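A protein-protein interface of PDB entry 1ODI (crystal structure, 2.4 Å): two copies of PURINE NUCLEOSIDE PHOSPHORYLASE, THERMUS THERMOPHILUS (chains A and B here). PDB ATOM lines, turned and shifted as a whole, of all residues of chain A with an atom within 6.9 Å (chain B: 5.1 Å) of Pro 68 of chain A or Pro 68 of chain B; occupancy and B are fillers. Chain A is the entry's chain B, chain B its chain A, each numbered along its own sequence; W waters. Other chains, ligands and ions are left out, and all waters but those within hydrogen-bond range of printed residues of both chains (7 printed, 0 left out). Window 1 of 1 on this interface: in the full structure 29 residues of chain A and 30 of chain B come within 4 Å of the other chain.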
ATOM      1  N   THR A  63     -32.972  -3.573 -24.647  1.00  0.00           N
ATOM      2  CA  THR A  63     -32.237  -4.539 -23.831  1.00  0.00           C
ATOM      3  C   THR A  63     -30.902  -4.933 -24.425  1.00  0.00           C
ATOM      4  O   THR A  63     -29.978  -5.287 -23.701  1.00  0.00           O
ATOM      5  CB  THR A  63     -33.012  -5.854 -23.659  1.00  0.00           C
ATOM      6  OG1 THR A  63     -33.186  -6.466 -24.945  1.00  0.00           O
ATOM      7  CG2 THR A  63     -34.367  -5.614 -23.017  1.00  0.00           C
ATOM      8  N   MET A  65     -28.838  -7.415 -27.347  1.00  0.00           N
ATOM      9  CA  MET A  65     -28.993  -8.827 -27.646  1.00  0.00           C
ATOM     10  C   MET A  65     -28.300  -9.716 -26.628  1.00  0.00           C
ATOM     11  O   MET A  65     -27.220  -9.388 -26.136  1.00  0.00           O
ATOM     12  CB  MET A  65     -28.457  -9.135 -29.038  1.00  0.00           C
ATOM     13  CG  MET A  65     -29.128  -8.346 -30.144  1.00  0.00           C
ATOM     14  SD  MET A  65     -28.518  -8.865 -31.750  1.00  0.00           S
ATOM     15  CE  MET A  65     -26.822  -8.320 -31.660  1.00  0.00           C
ATOM     16  N   GLY A  66     -28.939 -10.846 -26.325  1.00  0.00           N
ATOM     17  CA  GLY A  66     -28.393 -11.798 -25.377  1.00  0.00           C
ATOM     18  C   GLY A  66     -28.923 -11.570 -23.977  1.00  0.00           C
ATOM     19  O   GLY A  66     -29.293 -10.452 -23.626  1.00  0.00           O
ATOM     20  N   THR A  67     -28.974 -12.625 -23.171  1.00  0.00           N
ATOM     21  CA  THR A  67     -29.459 -12.487 -21.810  1.00  0.00           C
ATOM     22  C   THR A  67     -28.473 -11.728 -20.924  1.00  0.00           C
ATOM     23  O   THR A  67     -28.867 -11.117 -19.936  1.00  0.00           O
ATOM     24  CB  THR A  67     -29.768 -13.856 -21.180  1.00  0.00           C
ATOM     25  OG1 THR A  67     -28.675 -14.747 -21.410  1.00  0.00           O
ATOM     26  CG2 THR A  67     -31.038 -14.444 -21.782  1.00  0.00           C
ATOM     27  N   PRO A  68     -27.173 -11.750 -21.262  1.00  0.00           N
ATOM     28  CA  PRO A  68     -26.263 -11.003 -20.390  1.00  0.00           C
ATOM     29  C   PRO A  68     -26.629  -9.524 -20.405  1.00  0.00           C
ATOM     30  O   PRO A  68     -26.711  -8.866 -19.363  1.00  0.00           O
ATOM     31  CB  PRO A  68     -24.896 -11.262 -21.017  1.00  0.00           C
ATOM     32  CG  PRO A  68     -25.049 -12.641 -21.608  1.00  0.00           C
ATOM     33  CD  PRO A  68     -26.419 -12.557 -22.242  1.00  0.00           C
ATOM     34  N   SER A  69     -26.859  -9.015 -21.610  1.00  0.00           N
ATOM     35  CA  SER A  69     -27.216  -7.620 -21.813  1.00  0.00           C
ATOM     36  C   SER A  69     -28.594  -7.334 -21.229  1.00  0.00           C
ATOM     37  O   SER A  69     -28.773  -6.368 -20.485  1.00  0.00           O
ATOM     38  CB  SER A  69     -27.209  -7.304 -23.311  1.00  0.00           C
ATOM     39  OG  SER A  69     -27.528  -5.948 -23.559  1.00  0.00           O
ATOM     40  N   ALA A  70     -29.556  -8.191 -21.561  1.00  0.00           N
ATOM     41  CA  ALA A  70     -30.932  -8.037 -21.100  1.00  0.00           C
ATOM     42  C   ALA A  70     -31.071  -8.104 -19.589  1.00  0.00           C
ATOM     43  O   ALA A  70     -31.857  -7.346 -19.006  1.00  0.00           O
ATOM     44  CB  ALA A  70     -31.823  -9.090 -21.752  1.00  0.00           C
ATOM     45  N   ALA A  71     -30.315  -8.999 -18.955  1.00  0.00           N
ATOM     46  CA  ALA A  71     -30.379  -9.143 -17.504  1.00  0.00           C
ATOM     47  C   ALA A  71     -29.963  -7.845 -16.832  1.00  0.00           C
ATOM     48  O   ALA A  71     -30.564  -7.425 -15.844  1.00  0.00           O
ATOM     49  CB  ALA A  71     -29.483 -10.287 -17.041  1.00  0.00           C
ATOM     50  N   ILE A  72     -28.930  -7.207 -17.372  1.00  0.00           N
ATOM     51  CA  ILE A  72     -28.456  -5.955 -16.816  1.00  0.00           C
ATOM     52  C   ILE A  72     -29.561  -4.915 -16.851  1.00  0.00           C
ATOM     53  O   ILE A  72     -29.857  -4.286 -15.838  1.00  0.00           O
ATOM     54  CB  ILE A  72     -27.227  -5.434 -17.588  1.00  0.00           C
ATOM     55  CG1 ILE A  72     -25.966  -6.150 -17.080  1.00  0.00           C
ATOM     56  CG2 ILE A  72     -27.112  -3.919 -17.438  1.00  0.00           C
ATOM     57  CD1 ILE A  72     -24.707  -5.782 -17.821  1.00  0.00           C
ATOM     58  N   VAL A  73     -30.178  -4.746 -18.017  1.00  0.00           N
ATOM     59  CA  VAL A  73     -31.252  -3.773 -18.184  1.00  0.00           C
ATOM     60  C   VAL A  73     -32.449  -4.043 -17.257  1.00  0.00           C
ATOM     61  O   VAL A  73     -32.996  -3.117 -16.650  1.00  0.00           O
ATOM     62  CB  VAL A  73     -31.715  -3.742 -19.655  1.00  0.00           C
ATOM     63  CG1 VAL A  73     -32.862  -2.759 -19.834  1.00  0.00           C
ATOM     64  CG2 VAL A  73     -30.548  -3.355 -20.541  1.00  0.00           C
ATOM     65  N   ASP A 113     -29.029 -20.589 -21.970  1.00  0.00           N
ATOM     66  CA  ASP A 113     -28.118 -19.475 -21.757  1.00  0.00           C
ATOM     67  C   ASP A 113     -27.377 -19.585 -20.433  1.00  0.00           C
ATOM     68  O   ASP A 113     -27.871 -20.186 -19.482  1.00  0.00           O
ATOM     69  CB  ASP A 113     -28.904 -18.169 -21.778  1.00  0.00           C
ATOM     70  CG  ASP A 113     -29.809 -18.023 -20.572  1.00  0.00           C
ATOM     71  OD1 ASP A 113     -29.584 -17.087 -19.772  1.00  0.00           O
ATOM     72  OD2 ASP A 113     -30.739 -18.848 -20.424  1.00  0.00           O
ATOM     73  N   GLY A 114     -26.195 -18.981 -20.370  1.00  0.00           N
ATOM     74  CA  GLY A 114     -25.408 -19.030 -19.148  1.00  0.00           C
ATOM     75  C   GLY A 114     -25.769 -17.991 -18.093  1.00  0.00           C
ATOM     76  O   GLY A 114     -25.309 -18.085 -16.952  1.00  0.00           O
ATOM     77  N   THR A 115     -26.582 -17.003 -18.470  1.00  0.00           N
ATOM     78  CA  THR A 115     -27.003 -15.953 -17.546  1.00  0.00           C
ATOM     79  C   THR A 115     -27.922 -16.549 -16.493  1.00  0.00           C
ATOM     80  O   THR A 115     -27.680 -16.403 -15.287  1.00  0.00           O
ATOM     81  CB  THR A 115     -27.744 -14.810 -18.286  1.00  0.00           C
ATOM     82  OG1 THR A 115     -26.892 -14.273 -19.302  1.00  0.00           O
ATOM     83  CG2 THR A 115     -28.120 -13.684 -17.323  1.00  0.00           C
ATOM     84  N   GLU A 156     -31.092 -18.788 -26.237  1.00  0.00           N
ATOM     85  CA  GLU A 156     -29.712 -19.239 -26.423  1.00  0.00           C
ATOM     86  C   GLU A 156     -28.698 -18.101 -26.367  1.00  0.00           C
ATOM     87  O   GLU A 156     -29.061 -16.938 -26.206  1.00  0.00           O
ATOM     88  CB  GLU A 156     -29.586 -19.947 -27.761  1.00  0.00           C
ATOM     89  CG  GLU A 156     -29.951 -19.060 -28.923  1.00  0.00           C
ATOM     90  CD  GLU A 156     -29.791 -19.756 -30.245  1.00  0.00           C
ATOM     91  OE1 GLU A 156     -30.134 -19.148 -31.274  1.00  0.00           O
ATOM     92  OE2 GLU A 156     -29.321 -20.913 -30.256  1.00  0.00           O
ATOM     93  N   ASP A 157     -27.424 -18.452 -26.511  1.00  0.00           N
ATOM     94  CA  ASP A 157     -26.331 -17.485 -26.476  1.00  0.00           C
ATOM     95  C   ASP A 157     -25.566 -17.434 -27.795  1.00  0.00           C
ATOM     96  O   ASP A 157     -25.158 -16.357 -28.236  1.00  0.00           O
ATOM     97  CB  ASP A 157     -25.352 -17.835 -25.354  1.00  0.00           C
ATOM     98  CG  ASP A 157     -25.897 -17.517 -23.979  1.00  0.00           C
ATOM     99  OD1 ASP A 157     -25.277 -17.946 -22.974  1.00  0.00           O
ATOM    100  OD2 ASP A 157     -26.937 -16.830 -23.903  1.00  0.00           O
ATOM    101  N   ALA A 158     -25.386 -18.597 -28.422  1.00  0.00           N
ATOM    102  CA  ALA A 158     -24.645 -18.684 -29.678  1.00  0.00           C
ATOM    103  C   ALA A 158     -25.524 -18.684 -30.922  1.00  0.00           C
ATOM    104  O   ALA A 158     -25.777 -19.733 -31.522  1.00  0.00           O
ATOM    105  CB  ALA A 158     -23.765 -19.912 -29.672  1.00  0.00           C
ATOM    106  N   PHE A 159     -25.975 -17.495 -31.309  1.00  0.00           N
ATOM    107  CA  PHE A 159     -26.816 -17.321 -32.484  1.00  0.00           C
ATOM    108  C   PHE A 159     -26.357 -18.221 -33.628  1.00  0.00           C
ATOM    109  O   PHE A 159     -27.155 -18.959 -34.204  1.00  0.00           O
ATOM    110  CB  PHE A 159     -26.767 -15.861 -32.948  1.00  0.00           C
ATOM    111  CG  PHE A 159     -27.656 -15.562 -34.131  1.00  0.00           C
ATOM    112  CD1 PHE A 159     -28.952 -15.103 -33.947  1.00  0.00           C
ATOM    113  CD2 PHE A 159     -27.195 -15.745 -35.431  1.00  0.00           C
ATOM    114  CE1 PHE A 159     -29.776 -14.828 -35.047  1.00  0.00           C
ATOM    115  CE2 PHE A 159     -28.013 -15.473 -36.534  1.00  0.00           C
ATOM    116  CZ  PHE A 159     -29.302 -15.014 -36.339  1.00  0.00           C
ATOM    117  N   MET A 180     -33.045 -14.803 -27.775  1.00  0.00           N
ATOM    118  CA  MET A 180     -31.932 -14.658 -26.828  1.00  0.00           C
ATOM    119  C   MET A 180     -32.128 -13.720 -25.627  1.00  0.00           C
ATOM    120  O   MET A 180     -31.190 -13.027 -25.231  1.00  0.00           O
ATOM    121  CB  MET A 180     -30.670 -14.209 -27.596  1.00  0.00           C
ATOM    122  CG  MET A 180     -30.261 -15.095 -28.785  1.00  0.00           C
ATOM    123  SD  MET A 180     -29.087 -14.289 -29.934  1.00  0.00           S
ATOM    124  CE  MET A 180     -27.563 -14.369 -28.933  1.00  0.00           C
ATOM    125  N   ALA A 184     -33.805 -15.258 -19.100  1.00  0.00           N
ATOM    126  CA  ALA A 184     -33.300 -14.407 -18.033  1.00  0.00           C
ATOM    127  C   ALA A 184     -34.377 -13.446 -17.523  1.00  0.00           C
ATOM    128  O   ALA A 184     -34.469 -13.186 -16.320  1.00  0.00           O
ATOM    129  CB  ALA A 184     -32.062 -13.629 -18.523  1.00  0.00           C
ATOM    130  N   MET B  65     -22.796  -5.634 -25.052  1.00  0.00           N
ATOM    131  CA  MET B  65     -22.354  -6.297 -23.828  1.00  0.00           C
ATOM    132  C   MET B  65     -22.738  -7.778 -23.812  1.00  0.00           C
ATOM    133  O   MET B  65     -23.866  -8.144 -24.148  1.00  0.00           O
ATOM    134  CB  MET B  65     -22.971  -5.623 -22.592  1.00  0.00           C
ATOM    135  CG  MET B  65     -22.710  -4.144 -22.470  1.00  0.00           C
ATOM    136  SD  MET B  65     -23.325  -3.446 -20.915  1.00  0.00           S
ATOM    137  CE  MET B  65     -25.128  -3.398 -21.257  1.00  0.00           C
ATOM    138  N   GLY B  66     -21.800  -8.624 -23.402  1.00  0.00           N
ATOM    139  CA  GLY B  66     -22.085 -10.045 -23.324  1.00  0.00           C
ATOM    140  C   GLY B  66     -21.565 -10.813 -24.510  1.00  0.00           C
ATOM    141  O   GLY B  66     -21.617 -10.326 -25.641  1.00  0.00           O
ATOM    142  N   THR B  67     -21.069 -12.017 -24.250  1.00  0.00           N
ATOM    143  CA  THR B  67     -20.518 -12.875 -25.294  1.00  0.00           C
ATOM    144  C   THR B  67     -21.520 -13.243 -26.382  1.00  0.00           C
ATOM    145  O   THR B  67     -21.132 -13.552 -27.508  1.00  0.00           O
ATOM    146  CB  THR B  67     -19.947 -14.166 -24.694  1.00  0.00           C
ATOM    147  OG1 THR B  67     -20.893 -14.725 -23.782  1.00  0.00           O
ATOM    148  CG2 THR B  67     -18.640 -13.884 -23.963  1.00  0.00           C
ATOM    149  N   PRO B  68     -22.825 -13.230 -26.062  1.00  0.00           N
ATOM    150  CA  PRO B  68     -23.782 -13.581 -27.113  1.00  0.00           C
ATOM    151  C   PRO B  68     -23.812 -12.500 -28.182  1.00  0.00           C
ATOM    152  O   PRO B  68     -23.902 -12.786 -29.377  1.00  0.00           O
ATOM    153  CB  PRO B  68     -25.103 -13.689 -26.354  1.00  0.00           C
ATOM    154  CG  PRO B  68     -24.661 -14.161 -24.999  1.00  0.00           C
ATOM    155  CD  PRO B  68     -23.475 -13.258 -24.742  1.00  0.00           C
ATOM    156  N   SER B  69     -23.737 -11.253 -27.733  1.00  0.00           N
ATOM    157  CA  SER B  69     -23.754 -10.107 -28.627  1.00  0.00           C
ATOM    158  C   SER B  69     -22.433 -10.065 -29.380  1.00  0.00           C
ATOM    159  O   SER B  69     -22.408 -10.031 -30.612  1.00  0.00           O
ATOM    160  CB  SER B  69     -23.945  -8.822 -27.812  1.00  0.00           C
ATOM    161  OG  SER B  69     -24.181  -7.705 -28.649  1.00  0.00           O
ATOM    162  N   ALA B  70     -21.335 -10.085 -28.629  1.00  0.00           N
ATOM    163  CA  ALA B  70     -19.997 -10.041 -29.217  1.00  0.00           C
ATOM    164  C   ALA B  70     -19.743 -11.184 -30.202  1.00  0.00           C
ATOM    165  O   ALA B  70     -19.095 -10.990 -31.232  1.00  0.00           O
ATOM    166  CB  ALA B  70     -18.935 -10.056 -28.106  1.00  0.00           C
ATOM    167  N   ALA B  71     -20.249 -12.373 -29.884  1.00  0.00           N
ATOM    168  CA  ALA B  71     -20.072 -13.528 -30.756  1.00  0.00           C
ATOM    169  C   ALA B  71     -20.765 -13.286 -32.098  1.00  0.00           C
ATOM    170  O   ALA B  71     -20.239 -13.625 -33.155  1.00  0.00           O
ATOM    171  CB  ALA B  71     -20.624 -14.779 -30.088  1.00  0.00           C
ATOM    172  N   ILE B  72     -21.954 -12.701 -32.053  1.00  0.00           N
ATOM    173  CA  ILE B  72     -22.688 -12.393 -33.278  1.00  0.00           C
ATOM    174  C   ILE B  72     -21.854 -11.404 -34.105  1.00  0.00           C
ATOM    175  O   ILE B  72     -21.696 -11.554 -35.320  1.00  0.00           O
ATOM    176  CB  ILE B  72     -24.062 -11.752 -32.951  1.00  0.00           C
ATOM    177  CG1 ILE B  72     -25.001 -12.814 -32.369  1.00  0.00           C
ATOM    178  CG2 ILE B  72     -24.656 -11.115 -34.193  1.00  0.00           C
ATOM    179  CD1 ILE B  72     -26.362 -12.282 -31.936  1.00  0.00           C
ATOM    180  N   THR B 115     -22.017 -18.683 -23.955  1.00  0.00           N
ATOM    181  CA  THR B 115     -21.783 -18.628 -25.393  1.00  0.00           C
ATOM    182  C   THR B 115     -20.666 -19.594 -25.782  1.00  0.00           C
ATOM    183  O   THR B 115     -20.832 -20.411 -26.689  1.00  0.00           O
ATOM    184  CB  THR B 115     -21.414 -17.201 -25.858  1.00  0.00           C
ATOM    185  OG1 THR B 115     -22.527 -16.323 -25.641  1.00  0.00           O
ATOM    186  CG2 THR B 115     -21.065 -17.199 -27.342  1.00  0.00           C
ATOM    187  N   ASP B 157     -21.552 -13.994 -17.545  1.00  0.00           N
ATOM    188  CA  ASP B 157     -22.834 -13.655 -18.152  1.00  0.00           C
ATOM    189  C   ASP B 157     -23.673 -12.752 -17.262  1.00  0.00           C
ATOM    190  O   ASP B 157     -24.352 -11.853 -17.749  1.00  0.00           O
ATOM    191  CB  ASP B 157     -23.645 -14.922 -18.444  1.00  0.00           C
ATOM    192  CG  ASP B 157     -23.240 -15.599 -19.733  1.00  0.00           C
ATOM    193  OD1 ASP B 157     -23.687 -16.743 -19.951  1.00  0.00           O
ATOM    194  OD2 ASP B 157     -22.488 -14.996 -20.530  1.00  0.00           O
ATOM    195  N   MET B 180     -17.144  -9.174 -19.812  1.00  0.00           N
ATOM    196  CA  MET B 180     -18.137 -10.003 -20.491  1.00  0.00           C
ATOM    197  C   MET B 180     -18.022 -10.245 -21.993  1.00  0.00           C
ATOM    198  O   MET B 180     -19.047 -10.344 -22.670  1.00  0.00           O
ATOM    199  CB  MET B 180     -19.529  -9.424 -20.212  1.00  0.00           C
ATOM    200  CG  MET B 180     -19.872  -9.273 -18.734  1.00  0.00           C
ATOM    201  SD  MET B 180     -21.387  -8.307 -18.455  1.00  0.00           S
ATOM    202  CE  MET B 180     -22.643  -9.448 -19.061  1.00  0.00           C
HETATM  203  O   HOH W   1     -25.334 -10.521 -24.664  1.00  0.00           O
HETATM  204  O   HOH W   2     -25.685  -4.764 -25.267  1.00  0.00           O
HETATM  205  O   HOH W   3     -26.438  -5.877 -27.852  1.00  0.00           O
HETATM  206  O   HOH W   4     -24.335 -15.265 -30.235  1.00  0.00           O
HETATM  207  O   HOH W   5     -25.833  -9.860 -17.034  1.00  0.00           O
HETATM  208  O   HOH W   6     -22.946 -16.246 -22.997  1.00  0.00           O
HETATM  209  O   HOH W   7     -26.177 -15.887 -21.262  1.00  0.00           O
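OD1 of Asp 157 of chain B sits close to N of Gly 114 of chain A (3.4 Å).
The backbone NH of Thr 115 of chain B is in hydrogen-bond range of the side-chain carboxylate of Asp 157 of chain A (3.5 Å).
The side-chain carboxylate (OD1) of Asp 157 of chain B sits at hydrogen-bond distance from the backbone NH (N) of Thr 115 of chain A.
Water W4 lies within hydrogen-bond range of the backbone carbonyl oxygen of Asp 157 of chain A (2.4 Å), the backbone carbonyl oxygen of Pro 68 of chain B (2.7 Å) and the backbone NH of Phe 159 of chain A (3.0 Å).
Water W7 lies within hydrogen-bond range of the side-chain hydroxyl of Thr 115 of chain A (2.6 Å), the side-chain hydroxyl of Thr 67 of chain A (2.7 Å), the side-chain carboxylate of Asp 157 of chain A (2.8 Å), the side-chain carboxylate of Asp 157 of chain B (2.9 Å) and the backbone NH of Gly 114 of chain A (3.2 Å).
Water W1 bridges O of Met 65 of chain A (2.6 Å) and O of Met 65 of chain B (2.8 Å).
Water W6 lies within hydrogen-bond range of OG1 of Thr 67 of chain B, OG1 of Thr 115 of chain B, OD2 of Asp 157 of chain B and OD1 of Asp 157 of chain A.
Water W2 bridges OG of Ser 69 of chain A and N of Met 65 of chain B.
Water W3 bridges the backbone NH (N) of Met 65 of chain A (2.9 Å) and the side-chain hydroxyl (OG) of Ser 69 of chain B (3.0 Å).
Of the 11 printed residues of chain B, 8 touch a printed residue of chain A.
Hydrophobic or aromatic side chains of chain B within 4 Å of the printed part of chain A: Pro 68, Ile 72 and Met 180.
Hydrophobic or aromatic side chains of chain A that line the printed part of chain B: Met 65, Pro 68, Phe 159 and Met 180.
Among the printed residues, no Asp or Glu carboxylate lies within 4 Å of a Lys or Arg side-chain nitrogen of the other chain.
Met 65 of chain A touches Ile 72 of chain B, but with the chains exchanged Ile 72 of chain A does not touch Met 65 of chain B (4.1 Å).
Pro 68 of chain A touches Asp 157 of chain B, and with the chains exchanged Asp 157 of chain A touches Pro 68 of chain B.
Thr 115 of chain A touches Asp 157 of chain B, and with the chains exchanged Asp 157 of chain A touches Thr 115 of chain B.
Met 180 of chain A touches Ile 72 of chain B, but with the chains exchanged Ile 72 of chain A does not touch Met 180 of chain B (4.2 Å).
11 positions are printed for both chains.
Of the 16 pairs that touch across the chains among the printed residues, 12 have their exchanged pair printed and touching as well.
Printed residues of chain B within 4 Å of Gly 66 of chain A: Pro 68 (3.9 Å).
Pro 68 of chain A touches just these residues of chain B: Gly 66, Pro 68, Asp 157 and Met 180.
Of the printed residues of chain B, Thr 115 of chain A touches Asp 157 (3.3 Å).
Of the printed residues of chain B, Met 180 of chain A touches Pro 68 and Ile 72.
Of the printed residues of chain A, Thr 115 of chain B touches Asp 157 (3.2 Å).
Printed residues of chain A within 4 Å of Met 180 of chain B: Pro 68.
The nearest residue of chain B that does not touch Pro 68 of chain A is Met 65 of chain B (4.5 Å).
The nearest residue of chain A that does not touch Pro 68 of chain B is Met 65 of chain A (4.8 Å).
CB of Ser 69 of chain B touches O of Met 65 of chain A, at 3.7 Å.
Met 65 of chain A touches Ile 72 of chain B (CE to CD1, 3.998 Å).
CB of Pro 68 of chain B touches CA of Gly 66 of chain A, at 3.9 Å.
Pro 68 of chain A touches Gly 66 of chain B (CB to CA, 3.8 Å).
Pro 68 of chain B touches Pro 68 of chain A (CD to CG, 3.6 Å).
Pro 68 of chain A touches Asp 157 of chain B.
Met 65 of chain B touches Ser 69 of chain A (O to CB, 3.5 Å).
Asp 157 of chain B touches Asp 157 of chain A.
Phe 159 of chain A touches Ile 72 of chain B.
Met 180 of chain A touches Pro 68 of chain B.
The backbone carbonyl oxygen (O) of Met 180 of chain A is in hydrogen-bond range of the backbone NH (N) of Thr 67 of chain A (3.1 Å).
The side-chain carboxylate (OD1) of Asp 157 of chain A is in hydrogen-bond range of the backbone NH (N) of Gly 114 of chain A (2.9 Å).
The backbone NH of Gly 66 of chain B sits close to the backbone carbonyl oxygen of Met 180 of chain B, at 3.3 Å.
The side-chain hydroxyl of Thr 67 of chain A sits at hydrogen-bond distance from the side-chain hydroxyl of Thr 115 of chain A (2.8 Å).
The backbone carbonyl oxygen (O) of Met 180 of chain A sits close to the backbone NH (N) of Gly 66 of chain A (3.3 Å).
The side-chain hydroxyl (OG1) of Thr 67 of chain B is in hydrogen-bond range of the side-chain hydroxyl (OG1) of Thr 115 of chain B, 2.9 Å away.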
